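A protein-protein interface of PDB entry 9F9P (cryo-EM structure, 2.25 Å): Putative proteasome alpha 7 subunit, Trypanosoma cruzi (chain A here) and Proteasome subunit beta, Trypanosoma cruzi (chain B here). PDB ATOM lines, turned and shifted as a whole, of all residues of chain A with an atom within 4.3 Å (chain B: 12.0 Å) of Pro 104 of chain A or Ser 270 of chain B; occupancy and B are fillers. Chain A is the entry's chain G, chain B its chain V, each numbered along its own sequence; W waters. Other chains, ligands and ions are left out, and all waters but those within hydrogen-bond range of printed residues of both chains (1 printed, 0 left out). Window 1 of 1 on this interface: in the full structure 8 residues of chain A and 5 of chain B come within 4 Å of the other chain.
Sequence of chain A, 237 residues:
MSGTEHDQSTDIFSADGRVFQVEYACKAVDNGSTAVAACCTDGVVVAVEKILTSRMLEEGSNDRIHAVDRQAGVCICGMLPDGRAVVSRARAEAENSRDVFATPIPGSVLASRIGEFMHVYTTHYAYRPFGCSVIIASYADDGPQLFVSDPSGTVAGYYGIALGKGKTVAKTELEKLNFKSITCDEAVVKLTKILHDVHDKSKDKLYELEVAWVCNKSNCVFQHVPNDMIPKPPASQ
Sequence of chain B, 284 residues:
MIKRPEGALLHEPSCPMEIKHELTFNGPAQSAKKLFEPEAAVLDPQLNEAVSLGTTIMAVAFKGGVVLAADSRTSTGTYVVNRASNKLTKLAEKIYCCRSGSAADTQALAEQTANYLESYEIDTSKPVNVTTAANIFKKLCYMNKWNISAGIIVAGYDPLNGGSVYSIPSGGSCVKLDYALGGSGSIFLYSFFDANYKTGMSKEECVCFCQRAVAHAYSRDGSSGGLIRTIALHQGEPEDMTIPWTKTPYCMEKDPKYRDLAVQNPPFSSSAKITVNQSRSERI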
ATOM      1  N   ARG A  70     -30.445  10.042  -6.493  1.00  0.00           N
ATOM      2  CA  ARG A  70     -31.648  10.803  -6.159  1.00  0.00           C
ATOM      3  C   ARG A  70     -32.357  11.310  -7.415  1.00  0.00           C
ATOM      4  O   ARG A  70     -33.578  11.256  -7.485  1.00  0.00           O
ATOM      5  CB  ARG A  70     -31.224  11.934  -5.229  1.00  0.00           C
ATOM      6  CG  ARG A  70     -32.395  12.718  -4.672  1.00  0.00           C
ATOM      7  CD  ARG A  70     -31.842  13.789  -3.766  1.00  0.00           C
ATOM      8  NE  ARG A  70     -32.558  15.023  -4.034  1.00  0.00           N
ATOM      9  CZ  ARG A  70     -33.563  15.430  -3.300  1.00  0.00           C
ATOM     10  NH1 ARG A  70     -34.286  16.458  -3.686  1.00  0.00           N
ATOM     11  NH2 ARG A  70     -33.885  14.730  -2.236  1.00  0.00           N
ATOM     12  N   GLN A  71     -31.574  11.755  -8.426  1.00  0.00           N
ATOM     13  CA  GLN A  71     -32.066  12.480  -9.595  1.00  0.00           C
ATOM     14  C   GLN A  71     -32.031  11.670 -10.892  1.00  0.00           C
ATOM     15  O   GLN A  71     -32.145  12.250 -11.963  1.00  0.00           O
ATOM     16  CB  GLN A  71     -31.245  13.773  -9.781  1.00  0.00           C
ATOM     17  CG  GLN A  71     -29.796  13.688 -10.229  1.00  0.00           C
ATOM     18  CD  GLN A  71     -28.810  12.831  -9.442  1.00  0.00           C
ATOM     19  OE1 GLN A  71     -28.888  12.633  -8.218  1.00  0.00           O
ATOM     20  NE2 GLN A  71     -27.784  12.354 -10.136  1.00  0.00           N
ATOM     21  N   SER A  97     -19.183   9.402  -8.058  1.00  0.00           N
ATOM     22  CA  SER A  97     -19.166  10.808  -8.396  1.00  0.00           C
ATOM     23  C   SER A  97     -19.445  11.665  -7.169  1.00  0.00           C
ATOM     24  O   SER A  97     -18.852  12.726  -7.020  1.00  0.00           O
ATOM     25  CB  SER A  97     -20.116  11.120  -9.510  1.00  0.00           C
ATOM     26  OG  SER A  97     -20.431  12.491  -9.520  1.00  0.00           O
ATOM     27  N   ARG A  98     -20.350  11.238  -6.297  1.00  0.00           N
ATOM     28  CA  ARG A  98     -20.625  11.998  -5.082  1.00  0.00           C
ATOM     29  C   ARG A  98     -19.459  11.941  -4.102  1.00  0.00           C
ATOM     30  O   ARG A  98     -19.126  12.963  -3.533  1.00  0.00           O
ATOM     31  CB  ARG A  98     -21.899  11.484  -4.410  1.00  0.00           C
ATOM     32  CG  ARG A  98     -23.136  12.087  -5.063  1.00  0.00           C
ATOM     33  CD  ARG A  98     -24.414  11.571  -4.511  1.00  0.00           C
ATOM     34  NE  ARG A  98     -25.494  12.090  -5.358  1.00  0.00           N
ATOM     35  CZ  ARG A  98     -26.235  13.150  -5.079  1.00  0.00           C
ATOM     36  NH1 ARG A  98     -25.874  13.977  -4.124  1.00  0.00           N
ATOM     37  NH2 ARG A  98     -27.308  13.408  -5.795  1.00  0.00           N
ATOM     38  N   THR A 103     -20.101  15.871  -6.655  1.00  0.00           N
ATOM     39  CA  THR A 103     -21.193  16.314  -7.522  1.00  0.00           C
ATOM     40  C   THR A 103     -22.175  15.153  -7.720  1.00  0.00           C
ATOM     41  O   THR A 103     -21.782  13.993  -7.706  1.00  0.00           O
ATOM     42  CB  THR A 103     -20.741  16.799  -8.937  1.00  0.00           C
ATOM     43  OG1 THR A 103     -19.594  16.162  -9.522  1.00  0.00           O
ATOM     44  CG2 THR A 103     -20.392  18.268  -8.985  1.00  0.00           C
ATOM     45  N   PRO A 104     -23.457  15.437  -7.999  1.00  0.00           N
ATOM     46  CA  PRO A 104     -24.327  14.479  -8.681  1.00  0.00           C
ATOM     47  C   PRO A 104     -23.828  14.224 -10.095  1.00  0.00           C
ATOM     48  O   PRO A 104     -23.459  15.156 -10.786  1.00  0.00           O
ATOM     49  CB  PRO A 104     -25.678  15.190  -8.751  1.00  0.00           C
ATOM     50  CG  PRO A 104     -25.557  16.294  -7.663  1.00  0.00           C
ATOM     51  CD  PRO A 104     -24.110  16.728  -7.735  1.00  0.00           C
ATOM     52  N   ILE A 105     -23.747  12.960 -10.505  1.00  0.00           N
ATOM     53  CA  ILE A 105     -23.190  12.622 -11.807  1.00  0.00           C
ATOM     54  C   ILE A 105     -24.049  13.294 -12.881  1.00  0.00           C
ATOM     55  O   ILE A 105     -25.277  13.199 -12.886  1.00  0.00           O
ATOM     56  CB  ILE A 105     -23.081  11.083 -11.949  1.00  0.00           C
ATOM     57  CG1 ILE A 105     -22.199  10.682 -13.130  1.00  0.00           C
ATOM     58  CG2 ILE A 105     -24.436  10.368 -12.011  1.00  0.00           C
ATOM     59  CD1 ILE A 105     -21.648   9.269 -13.027  1.00  0.00           C
ATOM     60  N   PRO A 106     -23.456  14.062 -13.803  1.00  0.00           N
ATOM     61  CA  PRO A 106     -24.204  14.579 -14.940  1.00  0.00           C
ATOM     62  C   PRO A 106     -24.780  13.444 -15.800  1.00  0.00           C
ATOM     63  O   PRO A 106     -24.167  12.394 -15.952  1.00  0.00           O
ATOM     64  CB  PRO A 106     -23.167  15.366 -15.750  1.00  0.00           C
ATOM     65  CG  PRO A 106     -22.029  15.639 -14.768  1.00  0.00           C
ATOM     66  CD  PRO A 106     -22.054  14.479 -13.798  1.00  0.00           C
ATOM     67  N   ALA A 140     -29.806  16.411 -13.477  1.00  0.00           N
ATOM     68  CA  ALA A 140     -28.786  17.036 -12.639  1.00  0.00           C
ATOM     69  C   ALA A 140     -28.468  18.441 -13.174  1.00  0.00           C
ATOM     70  O   ALA A 140     -29.324  19.071 -13.808  1.00  0.00           O
ATOM     71  CB  ALA A 140     -27.583  16.111 -12.582  1.00  0.00           C
ATOM     72  N   ASN A 219     -39.443  17.706  -7.447  1.00  0.00           N
ATOM     73  CA  ASN A 219     -38.232  18.273  -6.849  1.00  0.00           C
ATOM     74  C   ASN A 219     -36.952  17.633  -7.390  1.00  0.00           C
ATOM     75  O   ASN A 219     -35.991  17.444  -6.648  1.00  0.00           O
ATOM     76  CB  ASN A 219     -38.192  18.174  -5.318  1.00  0.00           C
ATOM     77  CG  ASN A 219     -38.994  19.275  -4.663  1.00  0.00           C
ATOM     78  OD1 ASN A 219     -38.670  20.457  -4.809  1.00  0.00           O
ATOM     79  ND2 ASN A 219     -40.063  18.889  -3.979  1.00  0.00           N
ATOM     80  N   CYS A 220     -36.972  17.289  -8.685  1.00  0.00           N
ATOM     81  CA  CYS A 220     -35.901  16.588  -9.346  1.00  0.00           C
ATOM     82  C   CYS A 220     -35.578  15.316  -8.556  1.00  0.00           C
ATOM     83  O   CYS A 220     -34.412  14.958  -8.427  1.00  0.00           O
ATOM     84  CB  CYS A 220     -34.692  17.519  -9.536  1.00  0.00           C
ATOM     85  SG  CYS A 220     -34.951  19.076 -10.480  1.00  0.00           S
ATOM     86  N   PRO B 266     -24.892  20.417   4.476  1.00  0.00           N
ATOM     87  CA  PRO B 266     -25.950  20.665   3.492  1.00  0.00           C
ATOM     88  C   PRO B 266     -26.827  19.432   3.296  1.00  0.00           C
ATOM     89  O   PRO B 266     -26.321  18.315   3.330  1.00  0.00           O
ATOM     90  CB  PRO B 266     -25.185  20.971   2.193  1.00  0.00           C
ATOM     91  CG  PRO B 266     -23.824  20.309   2.358  1.00  0.00           C
ATOM     92  CD  PRO B 266     -23.564  20.239   3.853  1.00  0.00           C
ATOM     93  N   PRO B 267     -28.132  19.600   3.033  1.00  0.00           N
ATOM     94  CA  PRO B 267     -29.035  18.461   2.801  1.00  0.00           C
ATOM     95  C   PRO B 267     -28.710  17.708   1.515  1.00  0.00           C
ATOM     96  O   PRO B 267     -28.086  18.257   0.605  1.00  0.00           O
ATOM     97  CB  PRO B 267     -30.434  19.111   2.690  1.00  0.00           C
ATOM     98  CG  PRO B 267     -30.145  20.523   2.203  1.00  0.00           C
ATOM     99  CD  PRO B 267     -28.781  20.891   2.769  1.00  0.00           C
ATOM    100  N   PHE B 268     -29.125  16.445   1.454  1.00  0.00           N
ATOM    101  CA  PHE B 268     -28.967  15.597   0.269  1.00  0.00           C
ATOM    102  C   PHE B 268     -29.737  16.188  -0.918  1.00  0.00           C
ATOM    103  O   PHE B 268     -30.920  16.482  -0.778  1.00  0.00           O
ATOM    104  CB  PHE B 268     -29.458  14.192   0.638  1.00  0.00           C
ATOM    105  CG  PHE B 268     -29.224  13.100  -0.365  1.00  0.00           C
ATOM    106  CD1 PHE B 268     -27.998  12.961  -1.002  1.00  0.00           C
ATOM    107  CD2 PHE B 268     -30.229  12.184  -0.643  1.00  0.00           C
ATOM    108  CE1 PHE B 268     -27.785  11.928  -1.913  1.00  0.00           C
ATOM    109  CE2 PHE B 268     -30.006  11.137  -1.533  1.00  0.00           C
ATOM    110  CZ  PHE B 268     -28.787  11.006  -2.161  1.00  0.00           C
ATOM    111  N   SER B 269     -29.075  16.439  -2.061  1.00  0.00           N
ATOM    112  CA  SER B 269     -29.742  17.188  -3.130  1.00  0.00           C
ATOM    113  C   SER B 269     -29.410  16.675  -4.534  1.00  0.00           C
ATOM    114  O   SER B 269     -28.456  15.925  -4.729  1.00  0.00           O
ATOM    115  CB  SER B 269     -29.438  18.689  -3.007  1.00  0.00           C
ATOM    116  OG  SER B 269     -28.292  19.072  -3.723  1.00  0.00           O
ATOM    117  N   SER B 270     -30.163  17.178  -5.523  1.00  0.00           N
ATOM    118  CA  SER B 270     -29.936  16.870  -6.939  1.00  0.00           C
ATOM    119  C   SER B 270     -28.985  17.868  -7.600  1.00  0.00           C
ATOM    120  O   SER B 270     -28.792  17.812  -8.802  1.00  0.00           O
ATOM    121  CB  SER B 270     -31.260  16.847  -7.688  1.00  0.00           C
ATOM    122  OG  SER B 270     -32.145  15.877  -7.120  1.00  0.00           O
ATOM    123  N   SER B 271     -28.439  18.823  -6.840  1.00  0.00           N
ATOM    124  CA  SER B 271     -27.518  19.800  -7.386  1.00  0.00           C
ATOM    125  C   SER B 271     -26.243  19.885  -6.541  1.00  0.00           C
ATOM    126  O   SER B 271     -26.212  19.467  -5.386  1.00  0.00           O
ATOM    127  CB  SER B 271     -28.177  21.165  -7.504  1.00  0.00           C
ATOM    128  OG  SER B 271     -27.263  22.123  -8.046  1.00  0.00           O
ATOM    129  N   ALA B 272     -25.189  20.485  -7.116  1.00  0.00           N
ATOM    130  CA  ALA B 272     -23.924  20.682  -6.410  1.00  0.00           C
ATOM    131  C   ALA B 272     -23.840  22.076  -5.775  1.00  0.00           C
ATOM    132  O   ALA B 272     -22.850  22.391  -5.106  1.00  0.00           O
ATOM    133  CB  ALA B 272     -22.777  20.456  -7.359  1.00  0.00           C
ATOM    134  N   LYS B 273     -24.872  22.889  -5.997  1.00  0.00           N
ATOM    135  CA  LYS B 273     -24.996  24.180  -5.357  1.00  0.00           C
ATOM    136  C   LYS B 273     -25.131  23.982  -3.846  1.00  0.00           C
ATOM    137  O   LYS B 273     -25.846  23.093  -3.405  1.00  0.00           O
ATOM    138  CB  LYS B 273     -26.186  24.924  -5.971  1.00  0.00           C
ATOM    139  CG  LYS B 273     -26.480  26.284  -5.359  1.00  0.00           C
ATOM    140  CD  LYS B 273     -27.300  27.187  -6.260  1.00  0.00           C
ATOM    141  CE  LYS B 273     -27.277  28.644  -5.831  1.00  0.00           C
ATOM    142  NZ  LYS B 273     -25.905  29.220  -5.823  1.00  0.00           N
ATOM    143  N   ILE B 274     -24.409  24.811  -3.082  1.00  0.00           N
ATOM    144  CA  ILE B 274     -24.390  24.818  -1.625  1.00  0.00           C
ATOM    145  C   ILE B 274     -25.155  26.043  -1.134  1.00  0.00           C
ATOM    146  O   ILE B 274     -24.927  27.154  -1.604  1.00  0.00           O
ATOM    147  CB  ILE B 274     -22.930  24.790  -1.119  1.00  0.00           C
ATOM    148  CG1 ILE B 274     -22.262  23.443  -1.421  1.00  0.00           C
ATOM    149  CG2 ILE B 274     -22.863  25.132   0.366  1.00  0.00           C
ATOM    150  CD1 ILE B 274     -20.792  23.354  -1.052  1.00  0.00           C
ATOM    151  N   THR B 275     -26.067  25.845  -0.189  1.00  0.00           N
ATOM    152  CA  THR B 275     -27.080  26.854   0.106  1.00  0.00           C
ATOM    153  C   THR B 275     -27.131  27.105   1.624  1.00  0.00           C
ATOM    154  O   THR B 275     -26.617  28.110   2.100  1.00  0.00           O
ATOM    155  CB  THR B 275     -28.414  26.423  -0.539  1.00  0.00           C
ATOM    156  OG1 THR B 275     -28.196  25.945  -1.869  1.00  0.00           O
ATOM    157  CG2 THR B 275     -29.438  27.538  -0.592  1.00  0.00           C
ATOM    158  N   VAL B 276     -27.699  26.148   2.369  1.00  0.00           N
ATOM    159  CA  VAL B 276     -28.013  26.262   3.792  1.00  0.00           C
ATOM    160  C   VAL B 276     -27.693  24.930   4.475  1.00  0.00           C
ATOM    161  O   VAL B 276     -27.527  23.922   3.792  1.00  0.00           O
ATOM    162  CB  VAL B 276     -29.498  26.632   4.016  1.00  0.00           C
ATOM    163  CG1 VAL B 276     -29.834  27.980   3.384  1.00  0.00           C
ATOM    164  CG2 VAL B 276     -30.469  25.539   3.531  1.00  0.00           C
ATOM    165  N   GLN B 278     -28.917  21.797   6.838  1.00  0.00           N
ATOM    166  CA  GLN B 278     -30.131  21.067   7.156  1.00  0.00           C
ATOM    167  C   GLN B 278     -30.534  21.333   8.612  1.00  0.00           C
ATOM    168  O   GLN B 278     -29.723  21.271   9.525  1.00  0.00           O
ATOM    169  CB  GLN B 278     -29.871  19.580   6.902  1.00  0.00           C
ATOM    170  CG  GLN B 278     -31.147  18.769   6.680  1.00  0.00           C
ATOM    171  CD  GLN B 278     -30.829  17.305   6.529  1.00  0.00           C
ATOM    172  OE1 GLN B 278     -29.675  16.906   6.351  1.00  0.00           O
ATOM    173  NE2 GLN B 278     -31.861  16.493   6.661  1.00  0.00           N
ATOM    174  N   GLU B 282     -35.581  14.651   7.178  1.00  0.00           N
ATOM    175  CA  GLU B 282     -36.400  14.496   5.978  1.00  0.00           C
ATOM    176  C   GLU B 282     -37.682  13.694   6.284  1.00  0.00           C
ATOM    177  O   GLU B 282     -37.817  12.572   5.756  1.00  0.00           O
ATOM    178  CB  GLU B 282     -35.555  13.920   4.839  1.00  0.00           C
ATOM    179  CG  GLU B 282     -34.833  15.005   4.041  1.00  0.00           C
ATOM    180  CD  GLU B 282     -35.723  15.852   3.134  1.00  0.00           C
ATOM    181  OE1 GLU B 282     -35.387  15.994   1.934  1.00  0.00           O
ATOM    182  OE2 GLU B 282     -36.757  16.362   3.618  1.00  0.00           O
HETATM  183  O   HOH W   1     -26.051  16.267  -2.000  1.00  0.00           O
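The side-chain hydroxyl (OG) of Ser 270 of chain B sits at hydrogen-bond distance from the guanidinium group (NE) of Arg 70 of chain A. NH2 of Arg 98 of chain A lies within hydrogen-bond range of O of Ser 269 of chain B (3.0 Å). O of Cys 220 of chain A is in hydrogen-bond range of OG of Ser 270 of chain B, at 2.8 Å.
NH2 of Arg 98 of chain A is in hydrogen-bond range of OE1 of Gln 71 of chain A, at 3.0 Å. The side-chain hydroxyl of Ser 97 of chain A is in hydrogen-bond range of the backbone carbonyl oxygen of Thr 103 of chain A (2.7 Å). The backbone carbonyl oxygen (O) of Thr 103 of chain A sits at hydrogen-bond distance from the backbone NH (N) of Arg 98 of chain A, 3.4 Å away. The backbone carbonyl oxygen (O) of Ser 271 of chain B sits at hydrogen-bond distance from the side-chain hydroxyl (OG) of Ser 269 of chain B, at 2.7 Å. OG of Ser 271 of chain B lies within hydrogen-bond range of N of Lys 273 of chain B (3.2 Å).
Among the printed residues, merely in contact across the chains: Arg 70 of chain A with Phe 268 of chain B (3.7 Å), Arg 70 of chain A with Ser 269 of chain B (3.6 Å), Gln 71 of chain A with Ser 270 of chain B (3.5 Å), Arg 98 of chain A with Phe 268 of chain B (3.6 Å), Thr 103 of chain A with Ala 272 of chain B (3.6 Å), Pro 104 of chain A with Ser 270 of chain B (3.8 Å), Pro 104 of chain A with Ser 271 of chain B (3.8 Å), Pro 104 of chain A with Ala 272 of chain B (3.96 Å) and Ala 140 of chain A with Ser 270 of chain B (3.9 Å).
Pro 104 of chain A touches just these residues of chain B: Ser 270, Ser 271 and Ala 272. Of the printed residues of chain A, Ser 270 of chain B touches Arg 70 (3.2 Å), Gln 71 (3.5 Å), Pro 104 (3.8 Å), Ala 140 (3.9 Å) and Cys 220 (2.8 Å). Arg 70 of chain A touches just these residues of chain B: Phe 268 (3.7 Å), Ser 269 (3.6 Å) and Ser 270 (3.2 Å). Of chain B, only Ser 270 comes within 4 Å of Gln 71 of chain A. Printed residues of chain B within 4 Å of Thr 103 of chain A: Ala 272 (3.6 Å). No residue of chain B comes within 4 Å of Ile 105 of chain A. No residue of chain B comes within 4 Å of Pro 106 of chain A. Of the printed residues of chain B, Cys 220 of chain A touches Ser 270 (2.8 Å). Of the printed residues of chain A, Ser 271 of chain B touches Pro 104. Of the printed residues of chain A, Phe 268 of chain B touches Arg 70 and Arg 98. The nearest residue of chain A that does not touch Ser 270 of chain B is Asn 219 of chain A (4.2 Å).
Printed residues of chain A that touch a printed residue of chain B: Arg 70, Gln 71, Arg 98, Thr 103, Pro 104, Ala 140 and Cys 220. Of the 13 printed residues of chain B, 5 touch a printed residue of chain A. Printed residues of chain B that touch a printed residue of chain A: Phe 268, Ser 269, Ser 270, Ser 271 and Ala 272. Hydrophobic or aromatic side chains of chain B that line the printed part of chain A: Phe 268 and Ala 272. Among the printed residues, no Asp or Glu carboxylate lies within 4 Å of a Lys or Arg side-chain nitrogen of the other chain.
Water W1 bridges N of Ser 269 of chain B and NH1 of Arg 98 of chain A.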
